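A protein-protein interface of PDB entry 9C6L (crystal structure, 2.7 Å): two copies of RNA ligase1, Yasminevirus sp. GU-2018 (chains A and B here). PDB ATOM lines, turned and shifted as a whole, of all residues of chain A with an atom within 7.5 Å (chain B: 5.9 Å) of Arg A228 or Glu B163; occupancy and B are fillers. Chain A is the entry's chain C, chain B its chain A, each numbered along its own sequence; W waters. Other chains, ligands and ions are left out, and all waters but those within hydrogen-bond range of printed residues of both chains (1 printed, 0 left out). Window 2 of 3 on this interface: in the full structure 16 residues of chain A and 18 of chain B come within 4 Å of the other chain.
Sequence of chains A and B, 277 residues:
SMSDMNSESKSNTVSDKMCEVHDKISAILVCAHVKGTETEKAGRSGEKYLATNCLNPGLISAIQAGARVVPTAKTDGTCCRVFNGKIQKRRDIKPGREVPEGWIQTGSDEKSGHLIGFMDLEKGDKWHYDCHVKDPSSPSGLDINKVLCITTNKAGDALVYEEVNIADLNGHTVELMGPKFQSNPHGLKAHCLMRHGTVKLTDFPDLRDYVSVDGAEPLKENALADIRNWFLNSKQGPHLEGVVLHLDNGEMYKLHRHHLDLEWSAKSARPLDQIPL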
ATOM      1  N   LEU A  29     -11.239 -39.294  25.481  1.00  0.00           N
ATOM      2  CA  LEU A  29     -12.563 -38.715  25.622  1.00  0.00           C
ATOM      3  C   LEU A  29     -13.570 -39.558  24.853  1.00  0.00           C
ATOM      4  O   LEU A  29     -13.249 -40.140  23.811  1.00  0.00           O
ATOM      5  CB  LEU A  29     -12.591 -37.271  25.104  1.00  0.00           C
ATOM      6  CG  LEU A  29     -11.527 -36.334  25.678  1.00  0.00           C
ATOM      7  CD1 LEU A  29     -11.553 -34.992  24.962  1.00  0.00           C
ATOM      8  CD2 LEU A  29     -11.723 -36.149  27.173  1.00  0.00           C
ATOM      9  N   PHE A 204       1.475 -30.780  28.639  1.00  0.00           N
ATOM     10  CA  PHE A 204       0.210 -31.348  28.204  1.00  0.00           C
ATOM     11  C   PHE A 204      -0.814 -31.240  29.332  1.00  0.00           C
ATOM     12  O   PHE A 204      -0.462 -31.400  30.505  1.00  0.00           O
ATOM     13  CB  PHE A 204       0.384 -32.809  27.790  1.00  0.00           C
ATOM     14  CG  PHE A 204      -0.825 -33.396  27.119  1.00  0.00           C
ATOM     15  CD1 PHE A 204      -0.984 -33.307  25.746  1.00  0.00           C
ATOM     16  CD2 PHE A 204      -1.808 -34.026  27.862  1.00  0.00           C
ATOM     17  CE1 PHE A 204      -2.097 -33.841  25.126  1.00  0.00           C
ATOM     18  CE2 PHE A 204      -2.924 -34.561  27.247  1.00  0.00           C
ATOM     19  CZ  PHE A 204      -3.067 -34.468  25.876  1.00  0.00           C
ATOM     20  N   PRO A 205      -2.090 -30.959  29.016  1.00  0.00           N
ATOM     21  CA  PRO A 205      -3.093 -30.817  30.080  1.00  0.00           C
ATOM     22  C   PRO A 205      -3.105 -31.983  31.056  1.00  0.00           C
ATOM     23  O   PRO A 205      -3.305 -33.136  30.660  1.00  0.00           O
ATOM     24  CB  PRO A 205      -4.413 -30.726  29.303  1.00  0.00           C
ATOM     25  CG  PRO A 205      -4.033 -30.137  28.000  1.00  0.00           C
ATOM     26  CD  PRO A 205      -2.658 -30.666  27.686  1.00  0.00           C
ATOM     27  N   ASN A 222     -13.143 -28.452  30.681  1.00  0.00           N
ATOM     28  CA  ASN A 222     -13.150 -28.427  29.220  1.00  0.00           C
ATOM     29  C   ASN A 222     -11.922 -29.166  28.694  1.00  0.00           C
ATOM     30  O   ASN A 222     -11.005 -28.577  28.117  1.00  0.00           O
ATOM     31  CB  ASN A 222     -13.202 -26.980  28.715  1.00  0.00           C
ATOM     32  CG  ASN A 222     -14.516 -26.297  29.045  1.00  0.00           C
ATOM     33  OD1 ASN A 222     -15.572 -26.934  29.067  1.00  0.00           O
ATOM     34  ND2 ASN A 222     -14.460 -24.997  29.307  1.00  0.00           N
ATOM     35  N   ALA A 223     -11.922 -30.487  28.885  1.00  0.00           N
ATOM     36  CA  ALA A 223     -10.773 -31.293  28.481  1.00  0.00           C
ATOM     37  C   ALA A 223     -10.591 -31.286  26.969  1.00  0.00           C
ATOM     38  O   ALA A 223      -9.457 -31.293  26.475  1.00  0.00           O
ATOM     39  CB  ALA A 223     -10.933 -32.724  28.994  1.00  0.00           C
ATOM     40  N   LEU A 224     -11.693 -31.279  26.216  1.00  0.00           N
ATOM     41  CA  LEU A 224     -11.597 -31.284  24.760  1.00  0.00           C
ATOM     42  C   LEU A 224     -10.914 -30.019  24.252  1.00  0.00           C
ATOM     43  O   LEU A 224      -9.909 -30.080  23.535  1.00  0.00           O
ATOM     44  CB  LEU A 224     -12.992 -31.427  24.147  1.00  0.00           C
ATOM     45  CG  LEU A 224     -13.071 -31.402  22.617  1.00  0.00           C
ATOM     46  CD1 LEU A 224     -12.330 -32.585  22.014  1.00  0.00           C
ATOM     47  CD2 LEU A 224     -14.521 -31.383  22.155  1.00  0.00           C
ATOM     48  N   ALA A 225     -11.455 -28.854  24.618  1.00  0.00           N
ATOM     49  CA  ALA A 225     -10.900 -27.597  24.131  1.00  0.00           C
ATOM     50  C   ALA A 225      -9.451 -27.424  24.569  1.00  0.00           C
ATOM     51  O   ALA A 225      -8.600 -27.013  23.770  1.00  0.00           O
ATOM     52  CB  ALA A 225     -11.751 -26.428  24.625  1.00  0.00           C
ATOM     53  N   ASP A 226      -9.150 -27.729  25.832  1.00  0.00           N
ATOM     54  CA  ASP A 226      -7.788 -27.558  26.330  1.00  0.00           C
ATOM     55  C   ASP A 226      -6.807 -28.424  25.549  1.00  0.00           C
ATOM     56  O   ASP A 226      -5.747 -27.953  25.121  1.00  0.00           O
ATOM     57  CB  ASP A 226      -7.732 -27.891  27.822  1.00  0.00           C
ATOM     58  CG  ASP A 226      -8.700 -27.059  28.641  1.00  0.00           C
ATOM     59  OD1 ASP A 226      -9.009 -25.922  28.227  1.00  0.00           O
ATOM     60  OD2 ASP A 226      -9.156 -27.547  29.696  1.00  0.00           O
ATOM     61  N   ILE A 227      -7.144 -29.701  25.357  1.00  0.00           N
ATOM     62  CA  ILE A 227      -6.282 -30.587  24.577  1.00  0.00           C
ATOM     63  C   ILE A 227      -6.177 -30.087  23.143  1.00  0.00           C
ATOM     64  O   ILE A 227      -5.083 -30.015  22.570  1.00  0.00           O
ATOM     65  CB  ILE A 227      -6.806 -32.033  24.633  1.00  0.00           C
ATOM     66  CG1 ILE A 227      -6.627 -32.606  26.041  1.00  0.00           C
ATOM     67  CG2 ILE A 227      -6.093 -32.896  23.598  1.00  0.00           C
ATOM     68  CD1 ILE A 227      -7.285 -33.954  26.243  1.00  0.00           C
ATOM     69  N   ARG A 228      -7.316 -29.737  22.543  1.00  0.00           N
ATOM     70  CA  ARG A 228      -7.300 -29.191  21.189  1.00  0.00           C
ATOM     71  C   ARG A 228      -6.394 -27.972  21.104  1.00  0.00           C
ATOM     72  O   ARG A 228      -5.619 -27.829  20.151  1.00  0.00           O
ATOM     73  CB  ARG A 228      -8.720 -28.836  20.752  1.00  0.00           C
ATOM     74  CG  ARG A 228      -8.840 -28.413  19.294  1.00  0.00           C
ATOM     75  CD  ARG A 228     -10.298 -28.293  18.882  1.00  0.00           C
ATOM     76  NE  ARG A 228     -10.463 -28.214  17.433  1.00  0.00           N
ATOM     77  CZ  ARG A 228     -10.852 -27.135  16.765  1.00  0.00           C
ATOM     78  NH1 ARG A 228     -11.138 -25.997  17.381  1.00  0.00           N
ATOM     79  NH2 ARG A 228     -10.966 -27.199  15.441  1.00  0.00           N
ATOM     80  N   ASN A 229      -6.474 -27.082  22.096  1.00  0.00           N
ATOM     81  CA  ASN A 229      -5.615 -25.903  22.096  1.00  0.00           C
ATOM     82  C   ASN A 229      -4.147 -26.280  22.239  1.00  0.00           C
ATOM     83  O   ASN A 229      -3.275 -25.586  21.700  1.00  0.00           O
ATOM     84  CB  ASN A 229      -6.022 -24.953  23.219  1.00  0.00           C
ATOM     85  CG  ASN A 229      -5.127 -23.738  23.301  1.00  0.00           C
ATOM     86  OD1 ASN A 229      -5.365 -22.732  22.634  1.00  0.00           O
ATOM     87  ND2 ASN A 229      -4.084 -23.825  24.117  1.00  0.00           N
ATOM     88  N   TRP A 230      -3.848 -27.362  22.962  1.00  0.00           N
ATOM     89  CA  TRP A 230      -2.460 -27.790  23.085  1.00  0.00           C
ATOM     90  C   TRP A 230      -1.907 -28.276  21.751  1.00  0.00           C
ATOM     91  O   TRP A 230      -0.723 -28.077  21.464  1.00  0.00           O
ATOM     92  CB  TRP A 230      -2.330 -28.890  24.139  1.00  0.00           C
ATOM     93  CG  TRP A 230      -0.914 -29.335  24.340  1.00  0.00           C
ATOM     94  CD1 TRP A 230      -0.018 -28.834  25.240  1.00  0.00           C
ATOM     95  CD2 TRP A 230      -0.224 -30.364  23.619  1.00  0.00           C
ATOM     96  NE1 TRP A 230       1.185 -29.489  25.125  1.00  0.00           N
ATOM     97  CE2 TRP A 230       1.084 -30.432  24.137  1.00  0.00           C
ATOM     98  CE3 TRP A 230      -0.588 -31.234  22.587  1.00  0.00           C
ATOM     99  CZ2 TRP A 230       2.029 -31.337  23.659  1.00  0.00           C
ATOM    100  CZ3 TRP A 230       0.352 -32.132  22.114  1.00  0.00           C
ATOM    101  CH2 TRP A 230       1.646 -32.176  22.649  1.00  0.00           C
ATOM    102  N   PHE A 231      -2.742 -28.913  20.928  1.00  0.00           N
ATOM    103  CA  PHE A 231      -2.303 -29.347  19.608  1.00  0.00           C
ATOM    104  C   PHE A 231      -2.229 -28.200  18.609  1.00  0.00           C
ATOM    105  O   PHE A 231      -1.496 -28.306  17.621  1.00  0.00           O
ATOM    106  CB  PHE A 231      -3.236 -30.434  19.069  1.00  0.00           C
ATOM    107  CG  PHE A 231      -2.942 -31.800  19.614  1.00  0.00           C
ATOM    108  CD1 PHE A 231      -1.954 -32.585  19.046  1.00  0.00           C
ATOM    109  CD2 PHE A 231      -3.645 -32.296  20.699  1.00  0.00           C
ATOM    110  CE1 PHE A 231      -1.675 -33.842  19.546  1.00  0.00           C
ATOM    111  CE2 PHE A 231      -3.371 -33.553  21.204  1.00  0.00           C
ATOM    112  CZ  PHE A 231      -2.385 -34.327  20.625  1.00  0.00           C
ATOM    113  N   LEU A 232      -2.960 -27.113  18.847  1.00  0.00           N
ATOM    114  CA  LEU A 232      -2.953 -25.976  17.936  1.00  0.00           C
ATOM    115  C   LEU A 232      -1.828 -24.993  18.236  1.00  0.00           C
ATOM    116  O   LEU A 232      -1.253 -24.416  17.307  1.00  0.00           O
ATOM    117  CB  LEU A 232      -4.299 -25.244  17.999  1.00  0.00           C
ATOM    118  CG  LEU A 232      -5.487 -25.908  17.296  1.00  0.00           C
ATOM    119  CD1 LEU A 232      -6.782 -25.173  17.610  1.00  0.00           C
ATOM    120  CD2 LEU A 232      -5.261 -25.958  15.797  1.00  0.00           C
ATOM    121  N   ASN A 233      -1.488 -24.797  19.515  1.00  0.00           N
ATOM    122  CA  ASN A 233      -0.628 -23.691  19.908  1.00  0.00           C
ATOM    123  C   ASN A 233       0.561 -24.077  20.779  1.00  0.00           C
ATOM    124  O   ASN A 233       1.297 -23.181  21.209  1.00  0.00           O
ATOM    125  CB  ASN A 233      -1.455 -22.627  20.646  1.00  0.00           C
ATOM    126  CG  ASN A 233      -2.584 -22.082  19.796  1.00  0.00           C
ATOM    127  OD1 ASN A 233      -2.350 -21.436  18.775  1.00  0.00           O
ATOM    128  ND2 ASN A 233      -3.817 -22.337  20.217  1.00  0.00           N
ATOM    129  N   SER A 234       0.781 -25.359  21.050  1.00  0.00           N
ATOM    130  CA  SER A 234       1.973 -25.760  21.781  1.00  0.00           C
ATOM    131  C   SER A 234       3.160 -25.847  20.823  1.00  0.00           C
ATOM    132  O   SER A 234       3.032 -25.668  19.608  1.00  0.00           O
ATOM    133  CB  SER A 234       1.745 -27.091  22.494  1.00  0.00           C
ATOM    134  OG  SER A 234       1.622 -28.154  21.564  1.00  0.00           O
ATOM    135  N   LEU A 255      -5.643 -40.157  21.544  1.00  0.00           N
ATOM    136  CA  LEU A 255      -6.479 -39.176  20.861  1.00  0.00           C
ATOM    137  C   LEU A 255      -5.780 -38.769  19.574  1.00  0.00           C
ATOM    138  O   LEU A 255      -4.659 -38.254  19.612  1.00  0.00           O
ATOM    139  CB  LEU A 255      -6.745 -37.946  21.731  1.00  0.00           C
ATOM    140  CG  LEU A 255      -8.030 -37.927  22.563  1.00  0.00           C
ATOM    141  CD1 LEU A 255      -8.226 -36.552  23.180  1.00  0.00           C
ATOM    142  CD2 LEU A 255      -9.247 -38.316  21.740  1.00  0.00           C
ATOM    143  N   ARG A 257      -5.710 -36.487  15.935  1.00  0.00           N
ATOM    144  CA  ARG A 257      -6.101 -35.135  15.548  1.00  0.00           C
ATOM    145  C   ARG A 257      -7.527 -35.080  15.017  1.00  0.00           C
ATOM    146  O   ARG A 257      -8.139 -34.007  15.025  1.00  0.00           O
ATOM    147  CB  ARG A 257      -5.149 -34.584  14.488  1.00  0.00           C
ATOM    148  CG  ARG A 257      -3.911 -33.887  15.030  1.00  0.00           C
ATOM    149  CD  ARG A 257      -3.324 -32.966  13.969  1.00  0.00           C
ATOM    150  NE  ARG A 257      -1.952 -32.561  14.249  1.00  0.00           N
ATOM    151  CZ  ARG A 257      -1.213 -31.821  13.433  1.00  0.00           C
ATOM    152  NH1 ARG A 257      -1.691 -31.373  12.283  1.00  0.00           N
ATOM    153  NH2 ARG A 257       0.037 -31.525  13.776  1.00  0.00           N
ATOM    154  N   HIS A 259     -10.261 -36.730  16.202  1.00  0.00           N
ATOM    155  CA  HIS A 259     -11.158 -36.507  17.330  1.00  0.00           C
ATOM    156  C   HIS A 259     -11.235 -35.026  17.673  1.00  0.00           C
ATOM    157  O   HIS A 259     -12.299 -34.518  18.047  1.00  0.00           O
ATOM    158  CB  HIS A 259     -10.684 -37.300  18.547  1.00  0.00           C
ATOM    159  CG  HIS A 259     -10.580 -38.774  18.311  1.00  0.00           C
ATOM    160  ND1 HIS A 259      -9.483 -39.511  18.700  1.00  0.00           N
ATOM    161  CD2 HIS A 259     -11.439 -39.651  17.740  1.00  0.00           C
ATOM    162  CE1 HIS A 259      -9.666 -40.777  18.372  1.00  0.00           C
ATOM    163  NE2 HIS A 259     -10.846 -40.889  17.788  1.00  0.00           N
ATOM    164  N   LEU A 260     -10.113 -34.317  17.545  1.00  0.00           N
ATOM    165  CA  LEU A 260     -10.014 -32.905  17.882  1.00  0.00           C
ATOM    166  C   LEU A 260     -10.345 -31.997  16.703  1.00  0.00           C
ATOM    167  O   LEU A 260      -9.993 -30.811  16.728  1.00  0.00           O
ATOM    168  CB  LEU A 260      -8.610 -32.594  18.402  1.00  0.00           C
ATOM    169  CG  LEU A 260      -8.111 -33.544  19.493  1.00  0.00           C
ATOM    170  CD1 LEU A 260      -6.696 -33.191  19.919  1.00  0.00           C
ATOM    171  CD2 LEU A 260      -9.055 -33.518  20.683  1.00  0.00           C
ATOM    172  N   ASP A 261     -11.011 -32.525  15.675  1.00  0.00           N
ATOM    173  CA  ASP A 261     -11.407 -31.733  14.514  1.00  0.00           C
ATOM    174  C   ASP A 261     -10.212 -30.983  13.932  1.00  0.00           C
ATOM    175  O   ASP A 261     -10.303 -29.811  13.561  1.00  0.00           O
ATOM    176  CB  ASP A 261     -12.537 -30.767  14.881  1.00  0.00           C
ATOM    177  CG  ASP A 261     -13.130 -30.072  13.668  1.00  0.00           C
ATOM    178  OD1 ASP A 261     -13.609 -30.777  12.754  1.00  0.00           O
ATOM    179  OD2 ASP A 261     -13.120 -28.824  13.633  1.00  0.00           O
ATOM    180  N   LEU A 262      -9.072 -31.668  13.859  1.00  0.00           N
ATOM    181  CA  LEU A 262      -7.847 -31.104  13.318  1.00  0.00           C
ATOM    182  C   LEU A 262      -7.371 -31.928  12.130  1.00  0.00           C
ATOM    183  O   LEU A 262      -7.689 -33.112  11.992  1.00  0.00           O
ATOM    184  CB  LEU A 262      -6.740 -31.040  14.380  1.00  0.00           C
ATOM    185  CG  LEU A 262      -6.959 -30.062  15.537  1.00  0.00           C
ATOM    186  CD1 LEU A 262      -5.813 -30.141  16.537  1.00  0.00           C
ATOM    187  CD2 LEU A 262      -7.123 -28.640  15.023  1.00  0.00           C
ATOM    188  N   GLU A 263      -6.594 -31.274  11.272  1.00  0.00           N
ATOM    189  CA  GLU A 263      -6.074 -31.881  10.057  1.00  0.00           C
ATOM    190  C   GLU A 263      -4.720 -32.522  10.332  1.00  0.00           C
ATOM    191  O   GLU A 263      -3.890 -31.959  11.051  1.00  0.00           O
ATOM    192  CB  GLU A 263      -5.942 -30.819   8.962  1.00  0.00           C
ATOM    193  CG  GLU A 263      -5.400 -31.317   7.628  1.00  0.00           C
ATOM    194  CD  GLU A 263      -6.487 -31.787   6.681  1.00  0.00           C
ATOM    195  OE1 GLU A 263      -7.670 -31.808   7.086  1.00  0.00           O
ATOM    196  OE2 GLU A 263      -6.154 -32.131   5.527  1.00  0.00           O
ATOM    197  N   VAL B 133     -16.984 -24.008  15.905  1.00  0.00           N
ATOM    198  CA  VAL B 133     -16.617 -24.984  16.923  1.00  0.00           C
ATOM    199  C   VAL B 133     -17.699 -26.051  16.999  1.00  0.00           C
ATOM    200  O   VAL B 133     -18.895 -25.742  17.080  1.00  0.00           O
ATOM    201  CB  VAL B 133     -16.414 -24.299  18.283  1.00  0.00           C
ATOM    202  CG1 VAL B 133     -15.870 -25.292  19.302  1.00  0.00           C
ATOM    203  CG2 VAL B 133     -15.486 -23.099  18.147  1.00  0.00           C
ATOM    204  N   LYS B 134     -17.286 -27.315  16.973  1.00  0.00           N
ATOM    205  CA  LYS B 134     -18.240 -28.410  17.036  1.00  0.00           C
ATOM    206  C   LYS B 134     -18.911 -28.449  18.406  1.00  0.00           C
ATOM    207  O   LYS B 134     -18.302 -28.132  19.430  1.00  0.00           O
ATOM    208  CB  LYS B 134     -17.545 -29.738  16.743  1.00  0.00           C
ATOM    209  CG  LYS B 134     -16.771 -29.749  15.427  1.00  0.00           C
ATOM    210  CD  LYS B 134     -17.670 -29.443  14.232  1.00  0.00           C
ATOM    211  CE  LYS B 134     -16.872 -29.346  12.940  1.00  0.00           C
ATOM    212  NZ  LYS B 134     -15.936 -28.187  12.943  1.00  0.00           N
ATOM    213  N   LYS B 146     -19.855 -19.692  17.711  1.00  0.00           N
ATOM    214  CA  LYS B 146     -18.450 -19.886  18.044  1.00  0.00           C
ATOM    215  C   LYS B 146     -17.700 -20.310  16.789  1.00  0.00           C
ATOM    216  O   LYS B 146     -18.113 -21.252  16.107  1.00  0.00           O
ATOM    217  CB  LYS B 146     -18.286 -20.942  19.143  1.00  0.00           C
ATOM    218  CG  LYS B 146     -17.165 -20.654  20.133  1.00  0.00           C
ATOM    219  CD  LYS B 146     -17.505 -19.498  21.067  1.00  0.00           C
ATOM    220  CE  LYS B 146     -18.579 -19.878  22.078  1.00  0.00           C
ATOM    221  NZ  LYS B 146     -18.860 -18.767  23.031  1.00  0.00           N
ATOM    222  N   VAL B 147     -16.605 -19.612  16.490  1.00  0.00           N
ATOM    223  CA  VAL B 147     -15.771 -19.910  15.333  1.00  0.00           C
ATOM    224  C   VAL B 147     -14.323 -20.035  15.782  1.00  0.00           C
ATOM    225  O   VAL B 147     -13.913 -19.464  16.797  1.00  0.00           O
ATOM    226  CB  VAL B 147     -15.892 -18.832  14.232  1.00  0.00           C
ATOM    227  CG1 VAL B 147     -17.196 -18.990  13.470  1.00  0.00           C
ATOM    228  CG2 VAL B 147     -15.784 -17.438  14.834  1.00  0.00           C
ATOM    229  N   LEU B 148     -13.548 -20.794  15.013  1.00  0.00           N
ATOM    230  CA  LEU B 148     -12.110 -20.886  15.212  1.00  0.00           C
ATOM    231  C   LEU B 148     -11.428 -19.854  14.327  1.00  0.00           C
ATOM    232  O   LEU B 148     -11.678 -19.803  13.118  1.00  0.00           O
ATOM    233  CB  LEU B 148     -11.595 -22.287  14.884  1.00  0.00           C
ATOM    234  CG  LEU B 148     -10.098 -22.507  15.131  1.00  0.00           C
ATOM    235  CD1 LEU B 148      -9.787 -22.455  16.621  1.00  0.00           C
ATOM    236  CD2 LEU B 148      -9.634 -23.825  14.533  1.00  0.00           C
ATOM    237  N   CYS B 149     -10.576 -19.030  14.928  1.00  0.00           N
ATOM    238  CA  CYS B 149      -9.873 -17.986  14.204  1.00  0.00           C
ATOM    239  C   CYS B 149      -8.404 -17.997  14.592  1.00  0.00           C
ATOM    240  O   CYS B 149      -8.036 -18.436  15.685  1.00  0.00           O
ATOM    241  CB  CYS B 149     -10.468 -16.601  14.490  1.00  0.00           C
ATOM    242  SG  CYS B 149      -9.887 -15.864  16.032  1.00  0.00           S
ATOM    243  N   TYR B 161      -4.076 -20.019  17.345  1.00  0.00           N
ATOM    244  CA  TYR B 161      -5.457 -20.399  17.093  1.00  0.00           C
ATOM    245  C   TYR B 161      -6.270 -20.136  18.353  1.00  0.00           C
ATOM    246  O   TYR B 161      -5.848 -20.494  19.457  1.00  0.00           O
ATOM    247  CB  TYR B 161      -5.562 -21.875  16.709  1.00  0.00           C
ATOM    248  CG  TYR B 161      -4.749 -22.291  15.500  1.00  0.00           C
ATOM    249  CD1 TYR B 161      -3.397 -22.593  15.616  1.00  0.00           C
ATOM    250  CD2 TYR B 161      -5.341 -22.407  14.249  1.00  0.00           C
ATOM    251  CE1 TYR B 161      -2.656 -22.985  14.516  1.00  0.00           C
ATOM    252  CE2 TYR B 161      -4.608 -22.797  13.144  1.00  0.00           C
ATOM    253  CZ  TYR B 161      -3.267 -23.087  13.282  1.00  0.00           C
ATOM    254  OH  TYR B 161      -2.536 -23.476  12.183  1.00  0.00           O
ATOM    255  N   GLU B 162      -7.432 -19.507  18.194  1.00  0.00           N
ATOM    256  CA  GLU B 162      -8.274 -19.170  19.334  1.00  0.00           C
ATOM    257  C   GLU B 162      -9.734 -19.341  18.952  1.00  0.00           C
ATOM    258  O   GLU B 162     -10.170 -18.841  17.911  1.00  0.00           O
ATOM    259  CB  GLU B 162      -8.014 -17.734  19.808  1.00  0.00           C
ATOM    260  CG  GLU B 162      -8.654 -17.403  21.148  1.00  0.00           C
ATOM    261  CD  GLU B 162      -8.372 -15.981  21.599  1.00  0.00           C
ATOM    262  OE1 GLU B 162      -7.709 -15.235  20.848  1.00  0.00           O
ATOM    263  OE2 GLU B 162      -8.816 -15.609  22.706  1.00  0.00           O
ATOM    264  N   GLU B 163     -10.478 -20.057  19.791  1.00  0.00           N
ATOM    265  CA  GLU B 163     -11.922 -20.153  19.638  1.00  0.00           C
ATOM    266  C   GLU B 163     -12.563 -18.888  20.195  1.00  0.00           C
ATOM    267  O   GLU B 163     -12.317 -18.515  21.346  1.00  0.00           O
ATOM    268  CB  GLU B 163     -12.457 -21.388  20.358  1.00  0.00           C
ATOM    269  CG  GLU B 163     -11.905 -22.697  19.821  1.00  0.00           C
ATOM    270  CD  GLU B 163     -12.373 -23.898  20.616  1.00  0.00           C
ATOM    271  OE1 GLU B 163     -13.176 -23.712  21.555  1.00  0.00           O
ATOM    272  OE2 GLU B 163     -11.937 -25.027  20.301  1.00  0.00           O
ATOM    273  N   VAL B 164     -13.378 -18.224  19.375  1.00  0.00           N
ATOM    274  CA  VAL B 164     -13.912 -16.913  19.708  1.00  0.00           C
ATOM    275  C   VAL B 164     -15.413 -16.885  19.452  1.00  0.00           C
ATOM    276  O   VAL B 164     -15.956 -17.683  18.686  1.00  0.00           O
ATOM    277  CB  VAL B 164     -13.217 -15.790  18.906  1.00  0.00           C
ATOM    278  CG1 VAL B 164     -11.730 -15.760  19.223  1.00  0.00           C
ATOM    279  CG2 VAL B 164     -13.447 -15.981  17.413  1.00  0.00           C
ATOM    280  N   ASN B 165     -16.079 -15.943  20.115  1.00  0.00           N
ATOM    281  CA  ASN B 165     -17.488 -15.693  19.849  1.00  0.00           C
ATOM    282  C   ASN B 165     -17.627 -14.953  18.525  1.00  0.00           C
ATOM    283  O   ASN B 165     -17.013 -13.900  18.323  1.00  0.00           O
ATOM    284  CB  ASN B 165     -18.107 -14.878  20.983  1.00  0.00           C
ATOM    285  CG  ASN B 165     -19.619 -14.854  20.924  1.00  0.00           C
ATOM    286  OD1 ASN B 165     -20.211 -14.098  20.152  1.00  0.00           O
ATOM    287  ND2 ASN B 165     -20.256 -15.681  21.744  1.00  0.00           N
ATOM    288  N   ALA B 190      -6.383 -26.503  10.711  1.00  0.00           N
ATOM    289  CA  ALA B 190      -7.839 -26.574  10.737  1.00  0.00           C
ATOM    290  C   ALA B 190      -8.405 -25.356  10.023  1.00  0.00           C
ATOM    291  O   ALA B 190      -7.706 -24.363   9.801  1.00  0.00           O
ATOM    292  CB  ALA B 190      -8.384 -26.641  12.168  1.00  0.00           C
ATOM    293  N   HIS B 191      -9.685 -25.446   9.675  1.00  0.00           N
ATOM    294  CA  HIS B 191     -10.375 -24.342   9.022  1.00  0.00           C
ATOM    295  C   HIS B 191     -10.628 -23.228  10.027  1.00  0.00           C
ATOM    296  O   HIS B 191     -11.304 -23.437  11.039  1.00  0.00           O
ATOM    297  CB  HIS B 191     -11.683 -24.834   8.411  1.00  0.00           C
ATOM    298  CG  HIS B 191     -11.491 -25.783   7.271  1.00  0.00           C
ATOM    299  ND1 HIS B 191     -12.086 -27.026   7.226  1.00  0.00           N
ATOM    300  CD2 HIS B 191     -10.764 -25.672   6.134  1.00  0.00           C
ATOM    301  CE1 HIS B 191     -11.734 -27.639   6.110  1.00  0.00           C
ATOM    302  NE2 HIS B 191     -10.932 -26.839   5.430  1.00  0.00           N
HETATM  303  O   HOH W   1     -12.430 -25.844  12.421  1.00  0.00           O
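No position is printed for both chains.
Among the printed residues, pairs that only touch across the chains: Leu A232 with Tyr B161 (3.3 Å), Leu A262 with Ala B190 (3.7 Å), Arg A228 with Leu B148 (3.7 Å), Asn A229 with Tyr B161 (3.9 Å) and Asp A261 with Ala B190 (3.96 Å).
ND2 of Asn A233 lies within hydrogen-bond range of OD1 of Asn A229 (2.9 Å). O of Leu A260 sits at hydrogen-bond distance from NE of Arg A228, at 2.7 Å. NH2 of Arg A228 is in salt-bridge range of OD2 of Asp A261 (3.2 Å). The backbone carbonyl oxygen (O) of Arg A257 is in hydrogen-bond range of the backbone NH (N) of Leu A262 (2.8 Å).
Arg A228 touches two residues of chain B. Of the printed residues of chain B, Leu A232 touches Tyr B161. Of the printed residues of chain B, Asn A233 touches Tyr B161. Of the printed residues of chain B, Asp A261 touches Lys B134 (3.0 Å) and Ala B190 (3.96 Å). Of chain A, only Arg A228 comes within 4 Å of Glu B163. The nearest residue of chain B that does not touch Arg A228 is Ala B190 (4.2 Å). The nearest printed residue of chain B that does not touch Asn A233 is Glu B162 (5.0 Å).
Water W1 lies within hydrogen-bond range of O of His B191 and OD2 of Asp A261.
NH1 of Arg A228 is in salt-bridge range of OE2 of Glu B163 (3.2 Å). The backbone NH of Tyr B161 is in hydrogen-bond range of the side-chain amide oxygen of Asn A233. OD2 of Asp A261 is in salt-bridge range of NZ of Lys B134 (3.0 Å).
Printed residues of chain A that touch a printed residue of chain B: Arg A228, Asn A229, Leu A232, Asn A233, Asp A261 and Leu A262. Hydrophobic or aromatic side chains of chain B within 4 Å of the printed part of chain A: Leu B148, Tyr B161 and Ala B190. Among the printed residues, Asp or Glu carboxylates within 4 Å of a Lys or Arg side-chain nitrogen of the other chain: Arg A228 with Glu B163 and Asp A261 with Lys B134.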
